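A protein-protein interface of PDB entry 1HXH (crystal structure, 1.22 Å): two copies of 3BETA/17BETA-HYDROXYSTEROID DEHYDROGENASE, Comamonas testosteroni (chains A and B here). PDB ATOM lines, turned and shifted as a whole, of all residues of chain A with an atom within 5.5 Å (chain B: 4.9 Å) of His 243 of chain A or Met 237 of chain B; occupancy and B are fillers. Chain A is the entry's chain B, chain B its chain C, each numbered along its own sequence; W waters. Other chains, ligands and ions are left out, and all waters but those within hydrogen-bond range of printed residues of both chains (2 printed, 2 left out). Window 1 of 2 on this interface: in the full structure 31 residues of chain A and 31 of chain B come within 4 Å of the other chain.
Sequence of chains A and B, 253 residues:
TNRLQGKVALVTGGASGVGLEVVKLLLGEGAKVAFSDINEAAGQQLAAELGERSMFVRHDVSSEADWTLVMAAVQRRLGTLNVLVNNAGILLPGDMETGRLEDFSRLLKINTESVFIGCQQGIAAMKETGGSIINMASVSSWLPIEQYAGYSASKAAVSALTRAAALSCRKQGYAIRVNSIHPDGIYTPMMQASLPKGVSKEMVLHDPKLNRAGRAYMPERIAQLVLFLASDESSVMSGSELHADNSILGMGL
The backbone carbonyl oxygen (O) of His 182 of chain A lies within hydrogen-bond range of the backbone NH (N) of Ala 244 of chain A (3.0 Å).
The side-chain carboxylate of Glu 241 of chain A is in hydrogen-bond range of a ring nitrogen (NE2) of His 243 of chain A.
ND2 of Asn 179 of chain B lies within hydrogen-bond range of O of Met 237 of chain B (2.9 Å).
The backbone NH of Ser 238 of chain B sits close to the side-chain amide oxygen of Asn 179 of chain B (3.5 Å).
O of Phe 228 of chain B is in hydrogen-bond range of OG of Ser 234 of chain B (3.0 Å).
Water W2 bridges the backbone carbonyl oxygen (O) of Ser 235 of chain B (2.6 Å) and the side-chain amide oxygen (OD1) of Asn 246 of chain A (2.7 Å).
Water W1 bridges N of His 243 of chain A (2.9 Å) and OG of Ser 240 of chain B (2.9 Å).
Of the printed residues of chain B, His 243 of chain A touches Met 237 (3.3 Å).
Printed residues of chain A within 4 Å of Met 237 of chain B: Leu 225 (3.9 Å) and His 243 (3.3 Å).
Of the printed residues of chain A, Ser 238 of chain B touches Asp 245 and Asn 246.
Printed residues of chain B within 4 Å of Ala 244 of chain A: Val 236.
Printed residues of chain A within 4 Å of Val 236 of chain B: Leu 225, Ala 244, Asp 245 and Asn 246.
Printed residues of chain B within 4 Å of Asn 246 of chain A: Val 236 and Ser 238.
Leu 229 of chain B touches none of the printed residues of chain A.
The nearest printed residue of chain A that does not touch Met 237 of chain B is Leu 242 of chain A (4.04 Å).
The nearest printed residue of chain A that does not touch Ser 238 of chain B is His 243 of chain A (5.1 Å).
Among the printed residues, merely in contact across the chains: His 243 of chain A with Met 237 of chain B (3.3 Å), Asn 246 of chain A with Ser 238 of chain B (3.8 Å), Ala 244 of chain A with Val 236 of chain B (3.9 Å), Leu 225 of chain A with Met 237 of chain B (3.9 Å), Leu 225 of chain A with Phe 228 of chain B (3.9 Å), Asp 245 of chain A with Val 236 of chain B (3.9 Å), Leu 225 of chain A with Val 236 of chain B (3.9 Å) and Asp 245 of chain A with Ser 238 of chain B (3.95 Å).
The backbone NH of Asn 246 of chain A is in hydrogen-bond range of the backbone carbonyl oxygen of Val 236 of chain B (3.0 Å).
1 position is printed for both chains.
Of the 9 pairs that touch across the chains among the printed residues, none has its exchanged pair printed and touching as well.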
ATOM      1  N   TRP A 142      23.253   3.146   0.578  1.00  0.00           N
ATOM      2  CA  TRP A 142      23.693   1.754   0.415  1.00  0.00           C
ATOM      3  C   TRP A 142      24.750   1.586  -0.643  1.00  0.00           C
ATOM      4  O   TRP A 142      25.487   0.603  -0.599  1.00  0.00           O
ATOM      5  CB  TRP A 142      22.468   0.856   0.105  1.00  0.00           C
ATOM      6  CG  TRP A 142      21.714   1.192  -1.128  1.00  0.00           C
ATOM      7  CD1 TRP A 142      20.630   2.038  -1.292  1.00  0.00           C
ATOM      8  CD2 TRP A 142      22.005   0.683  -2.442  1.00  0.00           C
ATOM      9  NE1 TRP A 142      20.268   2.053  -2.572  1.00  0.00           N
ATOM     10  CE2 TRP A 142      21.056   1.254  -3.328  1.00  0.00           C
ATOM     11  CE3 TRP A 142      22.941  -0.191  -2.949  1.00  0.00           C
ATOM     12  CZ2 TRP A 142      21.062   0.945  -4.685  1.00  0.00           C
ATOM     13  CZ3 TRP A 142      22.962  -0.493  -4.284  1.00  0.00           C
ATOM     14  CH2 TRP A 142      22.019   0.083  -5.147  1.00  0.00           C
ATOM     15  N   SER A 180      11.375   5.634   3.468  1.00  0.00           N
ATOM     16  CA  SER A 180      12.415   6.483   2.896  1.00  0.00           C
ATOM     17  C   SER A 180      12.469   6.295   1.400  1.00  0.00           C
ATOM     18  O   SER A 180      12.097   5.253   0.849  1.00  0.00           O
ATOM     19  CB  SER A 180      13.771   6.176   3.552  1.00  0.00           C
ATOM     20  OG  SER A 180      14.165   4.830   3.429  1.00  0.00           O
ATOM     21  N   HIS A 182      15.151   6.748  -2.015  1.00  0.00           N
ATOM     22  CA  HIS A 182      16.598   6.747  -2.264  1.00  0.00           C
ATOM     23  C   HIS A 182      16.892   7.049  -3.740  1.00  0.00           C
ATOM     24  O   HIS A 182      17.095   6.123  -4.553  1.00  0.00           O
ATOM     25  CB  HIS A 182      17.195   5.379  -1.871  1.00  0.00           C
ATOM     26  CG  HIS A 182      16.964   5.067  -0.419  1.00  0.00           C
ATOM     27  ND1 HIS A 182      17.916   5.007   0.497  1.00  0.00           N
ATOM     28  CD2 HIS A 182      15.837   4.863   0.309  1.00  0.00           C
ATOM     29  CE1 HIS A 182      17.455   4.741   1.709  1.00  0.00           C
ATOM     30  NE2 HIS A 182      16.150   4.667   1.614  1.00  0.00           N
ATOM     31  N   LEU A 225       7.105   9.582  -6.420  1.00  0.00           N
ATOM     32  CA  LEU A 225       7.211   8.556  -5.361  1.00  0.00           C
ATOM     33  C   LEU A 225       6.728   9.096  -4.034  1.00  0.00           C
ATOM     34  O   LEU A 225       6.080   8.392  -3.260  1.00  0.00           O
ATOM     35  CB  LEU A 225       8.617   8.015  -5.237  1.00  0.00           C
ATOM     36  CG  LEU A 225       9.019   6.879  -6.177  1.00  0.00           C
ATOM     37  CD1 LEU A 225       8.821   7.250  -7.615  1.00  0.00           C
ATOM     38  CD2 LEU A 225      10.474   6.523  -5.907  1.00  0.00           C
ATOM     39  N   GLU A 241      12.463   1.050   2.323  1.00  0.00           N
ATOM     40  CA  GLU A 241      13.159   1.882   1.375  1.00  0.00           C
ATOM     41  C   GLU A 241      12.518   1.757  -0.003  1.00  0.00           C
ATOM     42  O   GLU A 241      12.351   0.656  -0.514  1.00  0.00           O
ATOM     43  CB  GLU A 241      14.627   1.463   1.256  1.00  0.00           C
ATOM     44  CG  GLU A 241      15.407   1.515   2.550  1.00  0.00           C
ATOM     45  CD  GLU A 241      16.889   1.413   2.409  1.00  0.00           C
ATOM     46  OE1 GLU A 241      17.399   1.078   1.328  1.00  0.00           O
ATOM     47  OE2 GLU A 241      17.627   1.695   3.390  1.00  0.00           O
ATOM     48  N   LEU A 242      12.174   2.888  -0.617  1.00  0.00           N
ATOM     49  CA  LEU A 242      11.802   2.862  -2.018  1.00  0.00           C
ATOM     50  C   LEU A 242      13.024   3.376  -2.760  1.00  0.00           C
ATOM     51  O   LEU A 242      13.522   4.469  -2.525  1.00  0.00           O
ATOM     52  CB  LEU A 242      10.594   3.711  -2.336  1.00  0.00           C
ATOM     53  CG  LEU A 242       9.240   3.274  -1.857  1.00  0.00           C
ATOM     54  CD1 LEU A 242       9.116   3.393  -0.354  1.00  0.00           C
ATOM     55  CD2 LEU A 242       8.160   4.094  -2.591  1.00  0.00           C
ATOM     56  N   HIS A 243      13.502   2.528  -3.644  1.00  0.00           N
ATOM     57  CA  HIS A 243      14.686   2.878  -4.392  1.00  0.00           C
ATOM     58  C   HIS A 243      14.309   3.529  -5.704  1.00  0.00           C
ATOM     59  O   HIS A 243      13.433   3.036  -6.420  1.00  0.00           O
ATOM     60  CB  HIS A 243      15.533   1.638  -4.646  1.00  0.00           C
ATOM     61  CG  HIS A 243      16.209   1.155  -3.390  1.00  0.00           C
ATOM     62  ND1 HIS A 243      17.126   0.128  -3.381  1.00  0.00           N
ATOM     63  CD2 HIS A 243      16.138   1.597  -2.117  1.00  0.00           C
ATOM     64  CE1 HIS A 243      17.563  -0.063  -2.148  1.00  0.00           C
ATOM     65  NE2 HIS A 243      16.976   0.819  -1.352  1.00  0.00           N
ATOM     66  N   ALA A 244      14.999   4.614  -6.038  1.00  0.00           N
ATOM     67  CA  ALA A 244      14.673   5.442  -7.190  1.00  0.00           C
ATOM     68  C   ALA A 244      15.949   5.693  -7.960  1.00  0.00           C
ATOM     69  O   ALA A 244      16.374   6.816  -8.197  1.00  0.00           O
ATOM     70  CB  ALA A 244      14.048   6.731  -6.727  1.00  0.00           C
ATOM     71  N   ASP A 245      16.590   4.586  -8.351  1.00  0.00           N
ATOM     72  CA  ASP A 245      17.901   4.655  -8.989  1.00  0.00           C
ATOM     73  C   ASP A 245      17.939   4.007 -10.351  1.00  0.00           C
ATOM     74  O   ASP A 245      19.013   3.948 -10.956  1.00  0.00           O
ATOM     75  CB  ASP A 245      18.958   4.012  -8.063  1.00  0.00           C
ATOM     76  CG  ASP A 245      18.628   2.558  -7.820  1.00  0.00           C
ATOM     77  OD1 ASP A 245      18.424   2.149  -6.665  1.00  0.00           O
ATOM     78  OD2 ASP A 245      18.547   1.782  -8.801  1.00  0.00           O
ATOM     79  N   ASN A 246      16.832   3.560 -10.894  1.00  0.00           N
ATOM     80  CA  ASN A 246      16.789   3.100 -12.260  1.00  0.00           C
ATOM     81  C   ASN A 246      17.829   2.043 -12.563  1.00  0.00           C
ATOM     82  O   ASN A 246      18.585   2.144 -13.537  1.00  0.00           O
ATOM     83  CB  ASN A 246      16.918   4.296 -13.241  1.00  0.00           C
ATOM     84  CG  ASN A 246      16.810   3.894 -14.673  1.00  0.00           C
ATOM     85  OD1 ASN A 246      16.052   3.026 -15.074  1.00  0.00           O
ATOM     86  ND2 ASN A 246      17.572   4.372 -15.611  1.00  0.00           N
ATOM     87  N   ARG B 177      11.078  -1.028 -17.213  1.00  0.00           N
ATOM     88  CA  ARG B 177      11.363  -1.151 -15.795  1.00  0.00           C
ATOM     89  C   ARG B 177      10.947  -2.549 -15.333  1.00  0.00           C
ATOM     90  O   ARG B 177       9.920  -3.059 -15.788  1.00  0.00           O
ATOM     91  CB  ARG B 177      10.627  -0.119 -14.940  1.00  0.00           C
ATOM     92  CG  ARG B 177      10.949   1.309 -15.337  1.00  0.00           C
ATOM     93  CD  ARG B 177       9.810   1.881 -16.217  1.00  0.00           C
ATOM     94  NE  ARG B 177       8.594   1.934 -15.445  1.00  0.00           N
ATOM     95  CZ  ARG B 177       7.412   2.332 -15.873  1.00  0.00           C
ATOM     96  NH1 ARG B 177       7.296   2.715 -17.150  1.00  0.00           N
ATOM     97  NH2 ARG B 177       6.372   2.347 -15.061  1.00  0.00           N
ATOM     98  N   ASN B 179      10.537  -4.645 -11.605  1.00  0.00           N
ATOM     99  CA  ASN B 179      10.563  -4.500 -10.150  1.00  0.00           C
ATOM    100  C   ASN B 179       9.758  -5.644  -9.558  1.00  0.00           C
ATOM    101  O   ASN B 179       8.980  -6.271 -10.225  1.00  0.00           O
ATOM    102  CB  ASN B 179       9.968  -3.172  -9.694  1.00  0.00           C
ATOM    103  CG  ASN B 179      10.756  -1.952 -10.200  1.00  0.00           C
ATOM    104  OD1 ASN B 179      11.812  -1.614  -9.614  1.00  0.00           O
ATOM    105  ND2 ASN B 179      10.211  -1.323 -11.203  1.00  0.00           N
ATOM    106  N   PHE B 228       0.652   1.353  -9.157  1.00  0.00           N
ATOM    107  CA  PHE B 228       1.687   2.352  -9.161  1.00  0.00           C
ATOM    108  C   PHE B 228       2.825   1.967 -10.106  1.00  0.00           C
ATOM    109  O   PHE B 228       3.250   2.766 -10.947  1.00  0.00           O
ATOM    110  CB  PHE B 228       2.196   2.598  -7.741  1.00  0.00           C
ATOM    111  CG  PHE B 228       3.350   3.600  -7.684  1.00  0.00           C
ATOM    112  CD1 PHE B 228       3.184   4.903  -8.067  1.00  0.00           C
ATOM    113  CD2 PHE B 228       4.581   3.170  -7.241  1.00  0.00           C
ATOM    114  CE1 PHE B 228       4.198   5.833  -8.028  1.00  0.00           C
ATOM    115  CE2 PHE B 228       5.628   4.073  -7.156  1.00  0.00           C
ATOM    116  CZ  PHE B 228       5.400   5.357  -7.548  1.00  0.00           C
ATOM    117  N   LEU B 229       3.303   0.762 -10.019  1.00  0.00           N
ATOM    118  CA  LEU B 229       4.401   0.335 -10.906  1.00  0.00           C
ATOM    119  C   LEU B 229       3.985   0.261 -12.359  1.00  0.00           C
ATOM    120  O   LEU B 229       4.846   0.434 -13.224  1.00  0.00           O
ATOM    121  CB  LEU B 229       4.939  -1.029 -10.430  1.00  0.00           C
ATOM    122  CG  LEU B 229       5.766  -0.984  -9.141  1.00  0.00           C
ATOM    123  CD1 LEU B 229       6.180  -2.394  -8.798  1.00  0.00           C
ATOM    124  CD2 LEU B 229       6.981  -0.064  -9.237  1.00  0.00           C
ATOM    125  N   SER B 234       5.762   5.941 -11.908  1.00  0.00           N
ATOM    126  CA  SER B 234       6.798   5.216 -11.163  1.00  0.00           C
ATOM    127  C   SER B 234       8.071   4.977 -11.964  1.00  0.00           C
ATOM    128  O   SER B 234       8.926   4.193 -11.512  1.00  0.00           O
ATOM    129  CB  SER B 234       6.262   3.860 -10.751  1.00  0.00           C
ATOM    130  OG  SER B 234       6.129   3.020 -11.871  1.00  0.00           O
ATOM    131  N   SER B 235       8.212   5.602 -13.141  1.00  0.00           N
ATOM    132  CA  SER B 235       9.210   5.101 -14.090  1.00  0.00           C
ATOM    133  C   SER B 235      10.658   5.202 -13.625  1.00  0.00           C
ATOM    134  O   SER B 235      11.455   4.486 -14.189  1.00  0.00           O
ATOM    135  CB  SER B 235       9.076   5.786 -15.429  1.00  0.00           C
ATOM    136  OG  SER B 235       9.279   7.154 -15.306  1.00  0.00           O
ATOM    137  N   VAL B 236      11.005   6.032 -12.636  1.00  0.00           N
ATOM    138  CA  VAL B 236      12.399   6.060 -12.196  1.00  0.00           C
ATOM    139  C   VAL B 236      12.785   4.805 -11.458  1.00  0.00           C
ATOM    140  O   VAL B 236      13.996   4.525 -11.298  1.00  0.00           O
ATOM    141  CB  VAL B 236      12.615   7.305 -11.341  1.00  0.00           C
ATOM    142  CG1 VAL B 236      11.977   7.163  -9.958  1.00  0.00           C
ATOM    143  CG2 VAL B 236      14.095   7.671 -11.210  1.00  0.00           C
ATOM    144  N   MET B 237      11.830   3.973 -11.032  1.00  0.00           N
ATOM    145  CA  MET B 237      12.081   2.772 -10.255  1.00  0.00           C
ATOM    146  C   MET B 237      12.347   1.570 -11.157  1.00  0.00           C
ATOM    147  O   MET B 237      11.461   1.162 -11.926  1.00  0.00           O
ATOM    148  CB  MET B 237      10.864   2.428  -9.366  1.00  0.00           C
ATOM    149  CG  MET B 237      10.594   3.530  -8.359  1.00  0.00           C
ATOM    150  SD  MET B 237       9.278   3.064  -7.235  1.00  0.00           S
ATOM    151  CE  MET B 237      10.319   2.156  -6.059  1.00  0.00           C
ATOM    152  N   SER B 238      13.561   0.982 -11.072  1.00  0.00           N
ATOM    153  CA  SER B 238      13.822  -0.244 -11.801  1.00  0.00           C
ATOM    154  C   SER B 238      14.843  -1.035 -11.062  1.00  0.00           C
ATOM    155  O   SER B 238      15.791  -0.486 -10.498  1.00  0.00           O
ATOM    156  CB  SER B 238      14.224   0.040 -13.257  1.00  0.00           C
ATOM    157  OG  SER B 238      14.177  -1.198 -13.927  1.00  0.00           O
ATOM    158  N   GLY B 239      14.693  -2.346 -11.070  1.00  0.00           N
ATOM    159  CA  GLY B 239      15.566  -3.250 -10.392  1.00  0.00           C
ATOM    160  C   GLY B 239      15.396  -3.337  -8.890  1.00  0.00           C
ATOM    161  O   GLY B 239      16.312  -3.839  -8.215  1.00  0.00           O
ATOM    162  N   SER B 240      14.242  -2.880  -8.409  1.00  0.00           N
ATOM    163  CA  SER B 240      14.047  -2.729  -6.973  1.00  0.00           C
ATOM    164  C   SER B 240      12.965  -3.674  -6.453  1.00  0.00           C
ATOM    165  O   SER B 240      12.154  -4.177  -7.199  1.00  0.00           O
ATOM    166  CB  SER B 240      13.705  -1.276  -6.691  1.00  0.00           C
ATOM    167  OG  SER B 240      12.282  -1.029  -6.840  1.00  0.00           O
ATOM    168  N   LEU B 242       9.816  -3.531  -3.867  1.00  0.00           N
ATOM    169  CA  LEU B 242       8.867  -2.726  -3.119  1.00  0.00           C
ATOM    170  C   LEU B 242       8.334  -3.650  -2.037  1.00  0.00           C
ATOM    171  O   LEU B 242       7.815  -4.720  -2.291  1.00  0.00           O
ATOM    172  CB  LEU B 242       7.746  -2.149  -3.965  1.00  0.00           C
ATOM    173  CG  LEU B 242       8.136  -1.043  -4.911  1.00  0.00           C
ATOM    174  CD1 LEU B 242       8.927  -1.561  -6.081  1.00  0.00           C
ATOM    175  CD2 LEU B 242       6.821  -0.369  -5.361  1.00  0.00           C
HETATM  176  O   HOH W   1      11.906   0.157  -4.174  1.00  0.00           O
HETATM  177  O   HOH W   2      13.529   3.816 -15.673  1.00  0.00           O
